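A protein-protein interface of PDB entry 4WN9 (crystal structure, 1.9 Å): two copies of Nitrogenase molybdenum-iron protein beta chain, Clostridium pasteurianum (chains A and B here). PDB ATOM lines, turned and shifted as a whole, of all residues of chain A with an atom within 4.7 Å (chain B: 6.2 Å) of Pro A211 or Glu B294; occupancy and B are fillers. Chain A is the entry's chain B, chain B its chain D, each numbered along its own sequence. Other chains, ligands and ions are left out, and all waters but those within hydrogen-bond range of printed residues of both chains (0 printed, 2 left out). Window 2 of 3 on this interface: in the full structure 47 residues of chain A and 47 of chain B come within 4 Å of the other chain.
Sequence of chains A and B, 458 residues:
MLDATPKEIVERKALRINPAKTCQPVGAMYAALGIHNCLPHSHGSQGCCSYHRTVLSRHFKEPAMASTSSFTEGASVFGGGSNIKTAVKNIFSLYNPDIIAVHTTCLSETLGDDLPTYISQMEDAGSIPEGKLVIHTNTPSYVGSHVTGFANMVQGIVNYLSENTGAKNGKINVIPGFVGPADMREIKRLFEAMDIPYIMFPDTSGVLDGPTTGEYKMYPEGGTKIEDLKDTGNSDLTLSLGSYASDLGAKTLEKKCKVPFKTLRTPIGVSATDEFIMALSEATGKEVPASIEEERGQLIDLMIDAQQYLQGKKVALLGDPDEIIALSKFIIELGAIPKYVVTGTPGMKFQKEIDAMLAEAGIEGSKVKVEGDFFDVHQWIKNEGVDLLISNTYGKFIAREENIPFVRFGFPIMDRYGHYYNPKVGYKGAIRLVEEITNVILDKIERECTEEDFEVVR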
ATOM      1  N   ARG A 185     -11.594  -3.957  38.282  1.00  0.00           N
ATOM      2  CA  ARG A 185     -11.243  -2.781  37.504  1.00  0.00           C
ATOM      3  C   ARG A 185     -10.502  -1.767  38.357  1.00  0.00           C
ATOM      4  O   ARG A 185      -9.489  -1.220  37.930  1.00  0.00           O
ATOM      5  CB  ARG A 185     -12.482  -2.104  36.915  1.00  0.00           C
ATOM      6  CG  ARG A 185     -13.189  -2.888  35.845  1.00  0.00           C
ATOM      7  CD  ARG A 185     -14.453  -2.188  35.410  1.00  0.00           C
ATOM      8  NE  ARG A 185     -15.208  -3.002  34.459  1.00  0.00           N
ATOM      9  CZ  ARG A 185     -15.128  -2.879  33.146  1.00  0.00           C
ATOM     10  NH1 ARG A 185     -14.311  -1.981  32.611  1.00  0.00           N
ATOM     11  NH2 ARG A 185     -15.871  -3.640  32.365  1.00  0.00           N
ATOM     12  N   GLY A 206     -15.198  -7.061  32.179  1.00  0.00           N
ATOM     13  CA  GLY A 206     -15.440  -7.248  30.776  1.00  0.00           C
ATOM     14  C   GLY A 206     -16.084  -8.584  30.472  1.00  0.00           C
ATOM     15  O   GLY A 206     -16.192  -8.978  29.298  1.00  0.00           O
ATOM     16  N   ASP A 209     -19.861  -7.750  33.455  1.00  0.00           N
ATOM     17  CA  ASP A 209     -20.247  -6.329  33.572  1.00  0.00           C
ATOM     18  C   ASP A 209     -20.195  -5.610  32.243  1.00  0.00           C
ATOM     19  O   ASP A 209     -19.973  -4.383  32.174  1.00  0.00           O
ATOM     20  CB  ASP A 209     -19.408  -5.601  34.615  1.00  0.00           C
ATOM     21  CG  ASP A 209     -17.951  -5.498  34.237  1.00  0.00           C
ATOM     22  OD1 ASP A 209     -17.506  -6.147  33.257  1.00  0.00           O
ATOM     23  OD2 ASP A 209     -17.252  -4.760  34.940  1.00  0.00           O
ATOM     24  N   GLY A 210     -20.514  -6.374  31.207  1.00  0.00           N
ATOM     25  CA  GLY A 210     -20.278  -5.989  29.838  1.00  0.00           C
ATOM     26  C   GLY A 210     -21.352  -5.196  29.145  1.00  0.00           C
ATOM     27  O   GLY A 210     -22.469  -5.071  29.638  1.00  0.00           O
ATOM     28  N   PRO A 211     -20.993  -4.623  27.982  1.00  0.00           N
ATOM     29  CA  PRO A 211     -21.895  -3.773  27.232  1.00  0.00           C
ATOM     30  C   PRO A 211     -22.917  -4.590  26.494  1.00  0.00           C
ATOM     31  O   PRO A 211     -22.716  -5.776  26.314  1.00  0.00           O
ATOM     32  CB  PRO A 211     -20.954  -3.024  26.263  1.00  0.00           C
ATOM     33  CG  PRO A 211     -19.789  -3.962  26.075  1.00  0.00           C
ATOM     34  CD  PRO A 211     -19.631  -4.666  27.408  1.00  0.00           C
ATOM     35  N   THR A 212     -24.024  -3.961  26.107  1.00  0.00           N
ATOM     36  CA  THR A 212     -24.921  -4.495  25.080  1.00  0.00           C
ATOM     37  C   THR A 212     -24.515  -3.825  23.742  1.00  0.00           C
ATOM     38  O   THR A 212     -24.560  -2.598  23.633  1.00  0.00           O
ATOM     39  CB  THR A 212     -26.404  -4.183  25.394  1.00  0.00           C
ATOM     40  OG1 THR A 212     -26.904  -5.080  26.406  1.00  0.00           O
ATOM     41  CG2 THR A 212     -27.276  -4.332  24.145  1.00  0.00           C
ATOM     42  N   THR A 213     -24.085  -4.618  22.758  1.00  0.00           N
ATOM     43  CA  THR A 213     -23.709  -4.088  21.448  1.00  0.00           C
ATOM     44  C   THR A 213     -24.699  -4.476  20.372  1.00  0.00           C
ATOM     45  O   THR A 213     -24.549  -4.070  19.229  1.00  0.00           O
ATOM     46  CB  THR A 213     -22.351  -4.615  20.958  1.00  0.00           C
ATOM     47  OG1 THR A 213     -22.429  -6.038  20.801  1.00  0.00           O
ATOM     48  CG2 THR A 213     -21.220  -4.235  21.913  1.00  0.00           C
ATOM     49  N   PRO B 289     -12.122   5.671  21.298  1.00  0.00           N
ATOM     50  CA  PRO B 289     -11.466   4.492  21.827  1.00  0.00           C
ATOM     51  C   PRO B 289     -12.416   3.482  22.460  1.00  0.00           C
ATOM     52  O   PRO B 289     -13.578   3.791  22.734  1.00  0.00           O
ATOM     53  CB  PRO B 289     -10.532   5.057  22.891  1.00  0.00           C
ATOM     54  CG  PRO B 289     -11.198   6.301  23.350  1.00  0.00           C
ATOM     55  CD  PRO B 289     -11.928   6.851  22.161  1.00  0.00           C
ATOM     56  N   ALA B 290     -11.893   2.292  22.710  1.00  0.00           N
ATOM     57  CA  ALA B 290     -12.694   1.173  23.158  1.00  0.00           C
ATOM     58  C   ALA B 290     -13.310   1.419  24.536  1.00  0.00           C
ATOM     59  O   ALA B 290     -14.461   1.070  24.771  1.00  0.00           O
ATOM     60  CB  ALA B 290     -11.840  -0.076  23.190  1.00  0.00           C
ATOM     61  N   SER B 291     -12.527   2.003  25.434  1.00  0.00           N
ATOM     62  CA  SER B 291     -12.976   2.287  26.781  1.00  0.00           C
ATOM     63  C   SER B 291     -14.259   3.106  26.793  1.00  0.00           C
ATOM     64  O   SER B 291     -15.165   2.806  27.561  1.00  0.00           O
ATOM     65  CB  SER B 291     -11.884   3.012  27.552  1.00  0.00           C
ATOM     66  OG  SER B 291     -11.845   4.368  27.176  1.00  0.00           O
ATOM     67  N   ILE B 292     -14.347   4.124  25.937  1.00  0.00           N
ATOM     68  CA  ILE B 292     -15.516   4.997  25.895  1.00  0.00           C
ATOM     69  C   ILE B 292     -16.694   4.290  25.271  1.00  0.00           C
ATOM     70  O   ILE B 292     -17.846   4.503  25.658  1.00  0.00           O
ATOM     71  CB  ILE B 292     -15.242   6.317  25.144  1.00  0.00           C
ATOM     72  CG1 ILE B 292     -14.417   7.259  26.015  1.00  0.00           C
ATOM     73  CG2 ILE B 292     -16.542   6.980  24.688  1.00  0.00           C
ATOM     74  CD1 ILE B 292     -13.991   8.543  25.315  1.00  0.00           C
ATOM     75  N   GLU B 293     -16.412   3.446  24.290  1.00  0.00           N
ATOM     76  CA  GLU B 293     -17.456   2.660  23.668  1.00  0.00           C
ATOM     77  C   GLU B 293     -17.996   1.652  24.682  1.00  0.00           C
ATOM     78  O   GLU B 293     -19.188   1.380  24.718  1.00  0.00           O
ATOM     79  CB  GLU B 293     -16.925   1.945  22.407  1.00  0.00           C
ATOM     80  CG  GLU B 293     -17.996   1.160  21.659  1.00  0.00           C
ATOM     81  CD  GLU B 293     -17.749   1.066  20.154  1.00  0.00           C
ATOM     82  OE1 GLU B 293     -16.646   1.437  19.675  1.00  0.00           O
ATOM     83  OE2 GLU B 293     -18.670   0.606  19.449  1.00  0.00           O
ATOM     84  N   GLU B 294     -17.125   1.077  25.494  1.00  0.00           N
ATOM     85  CA  GLU B 294     -17.602   0.126  26.482  1.00  0.00           C
ATOM     86  C   GLU B 294     -18.560   0.823  27.474  1.00  0.00           C
ATOM     87  O   GLU B 294     -19.630   0.292  27.780  1.00  0.00           O
ATOM     88  CB  GLU B 294     -16.465  -0.490  27.256  1.00  0.00           C
ATOM     89  CG  GLU B 294     -16.973  -1.578  28.181  1.00  0.00           C
ATOM     90  CD  GLU B 294     -15.952  -2.093  29.164  1.00  0.00           C
ATOM     91  OE1 GLU B 294     -15.179  -1.293  29.738  1.00  0.00           O
ATOM     92  OE2 GLU B 294     -15.967  -3.317  29.417  1.00  0.00           O
ATOM     93  N   GLU B 295     -18.163   1.988  27.989  1.00  0.00           N
ATOM     94  CA  GLU B 295     -19.024   2.752  28.914  1.00  0.00           C
ATOM     95  C   GLU B 295     -20.422   2.988  28.322  1.00  0.00           C
ATOM     96  O   GLU B 295     -21.438   2.786  28.997  1.00  0.00           O
ATOM     97  CB  GLU B 295     -18.414   4.109  29.240  1.00  0.00           C
ATOM     98  CG  GLU B 295     -17.022   4.105  29.870  1.00  0.00           C
ATOM     99  CD  GLU B 295     -16.389   5.499  29.864  1.00  0.00           C
ATOM    100  OE1 GLU B 295     -17.126   6.495  29.699  1.00  0.00           O
ATOM    101  OE2 GLU B 295     -15.155   5.607  30.010  1.00  0.00           O
ATOM    102  N   ARG B 296     -20.482   3.417  27.064  1.00  0.00           N
ATOM    103  CA  ARG B 296     -21.766   3.706  26.439  1.00  0.00           C
ATOM    104  C   ARG B 296     -22.595   2.437  26.411  1.00  0.00           C
ATOM    105  O   ARG B 296     -23.780   2.463  26.744  1.00  0.00           O
ATOM    106  CB  ARG B 296     -21.598   4.294  25.025  1.00  0.00           C
ATOM    107  CG  ARG B 296     -22.892   4.592  24.288  1.00  0.00           C
ATOM    108  CD  ARG B 296     -22.665   5.279  22.931  1.00  0.00           C
ATOM    109  NE  ARG B 296     -23.917   5.807  22.388  1.00  0.00           N
ATOM    110  CZ  ARG B 296     -24.907   5.088  21.877  1.00  0.00           C
ATOM    111  NH1 ARG B 296     -24.824   3.760  21.792  1.00  0.00           N
ATOM    112  NH2 ARG B 296     -25.998   5.701  21.437  1.00  0.00           N
ATOM    113  N   GLY B 297     -21.959   1.329  26.043  1.00  0.00           N
ATOM    114  CA  GLY B 297     -22.636   0.029  25.940  1.00  0.00           C
ATOM    115  C   GLY B 297     -23.124  -0.513  27.279  1.00  0.00           C
ATOM    116  O   GLY B 297     -24.149  -1.181  27.355  1.00  0.00           O
ATOM    117  N   GLN B 298     -22.385  -0.221  28.335  1.00  0.00           N
ATOM    118  CA  GLN B 298     -22.842  -0.527  29.690  1.00  0.00           C
ATOM    119  C   GLN B 298     -24.076   0.299  30.066  1.00  0.00           C
ATOM    120  O   GLN B 298     -24.986  -0.215  30.721  1.00  0.00           O
ATOM    121  CB  GLN B 298     -21.732  -0.282  30.677  1.00  0.00           C
ATOM    122  CG  GLN B 298     -20.600  -1.266  30.536  1.00  0.00           C
ATOM    123  CD  GLN B 298     -19.412  -0.861  31.350  1.00  0.00           C
ATOM    124  OE1 GLN B 298     -19.092   0.314  31.461  1.00  0.00           O
ATOM    125  NE2 GLN B 298     -18.754  -1.831  31.947  1.00  0.00           N
ATOM    126  N   LEU B 299     -24.110   1.565  29.650  1.00  0.00           N
ATOM    127  CA  LEU B 299     -25.264   2.402  29.891  1.00  0.00           C
ATOM    128  C   LEU B 299     -26.497   1.893  29.156  1.00  0.00           C
ATOM    129  O   LEU B 299     -27.589   1.803  29.739  1.00  0.00           O
ATOM    130  CB  LEU B 299     -24.997   3.841  29.453  1.00  0.00           C
ATOM    131  CG  LEU B 299     -26.249   4.736  29.442  1.00  0.00           C
ATOM    132  CD1 LEU B 299     -26.774   4.943  30.851  1.00  0.00           C
ATOM    133  CD2 LEU B 299     -25.934   6.077  28.785  1.00  0.00           C
ATOM    134  N   ASP B 301     -26.917  -1.147  28.150  1.00  0.00           N
ATOM    135  CA  ASP B 301     -27.226  -2.416  28.826  1.00  0.00           C
ATOM    136  C   ASP B 301     -28.076  -2.154  30.105  1.00  0.00           C
ATOM    137  O   ASP B 301     -29.071  -2.809  30.344  1.00  0.00           O
ATOM    138  CB  ASP B 301     -25.915  -3.112  29.180  1.00  0.00           C
ATOM    139  CG  ASP B 301     -26.117  -4.536  29.626  1.00  0.00           C
ATOM    140  OD1 ASP B 301     -26.415  -5.405  28.762  1.00  0.00           O
ATOM    141  OD2 ASP B 301     -25.989  -4.771  30.844  1.00  0.00           O
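The side-chain amide nitrogen (NE2) of Gln B298 lies close to the guanidinium group (NH2) of Arg A185, 3.4 Å away.
OE2 of Glu B294 lies within salt-bridge range of NH2 of Arg A185 (3.0 Å).
The backbone carbonyl oxygen (O) of Asp A209 lies within hydrogen-bond range of the side-chain amide nitrogen (NE2) of Gln B298, 2.8 Å away.
The backbone carbonyl oxygen (O) of Gly B297 lies within hydrogen-bond range of the backbone NH (N) of Thr A212 (3.0 Å).
OG1 of Thr A212 lies within hydrogen-bond range of OD1 of Asp B301, 2.4 Å away.
The guanidinium group (NE) of Arg A185 lies within salt-bridge range of the side-chain carboxylate (OD2) of Asp A209 (2.7 Å).
OD1 of Asp A209 is in hydrogen-bond range of N of Gly A206 (2.7 Å).
CG of Asp B301 touches O of Gly A210, at 3.7 Å.
Glu B294 touches Pro A211 (O to CB, 3.9 Å).
Pro A211 touches Gly B297.
Pro A211 touches Gln B298.
Gly A206 touches none of the printed residues of chain B.
Of chain B, only Glu B294, Gly B297 and Gln B298 come within 4 Å of Pro A211.
Glu B294 touches just these residues of chain A: Arg A185 and Pro A211.
Of the printed residues of chain A, Gly B297 touches Pro A211 and Thr A212.
Printed residues of chain A within 4 Å of Gln B298: Arg A185 (3.4 Å), Asp A209 (2.8 Å) and Pro A211 (3.8 Å).
Leu B299 touches none of the printed residues of chain A.
Of the printed residues of chain A, Asp B301 touches Gly A210 (3.7 Å) and Thr A212 (2.4 Å).
The nearest residue of chain B that does not touch Pro A211 is Asp B301 (4.2 Å).
The nearest residue of chain A that does not touch Glu B294 is Gly A206 (4.2 Å).
Printed residues of chain B that touch a printed residue of chain A: Glu B294, Gly B297, Gln B298 and Asp B301.
Of the 7 printed residues of chain A, 5 touch a printed residue of chain B.
Among the printed residues, 9 pairs touch across the chains.
No position is printed for both chains.
Of the 9 pairs that touch across the chains among the printed residues, none has its exchanged pair printed and touching as well.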
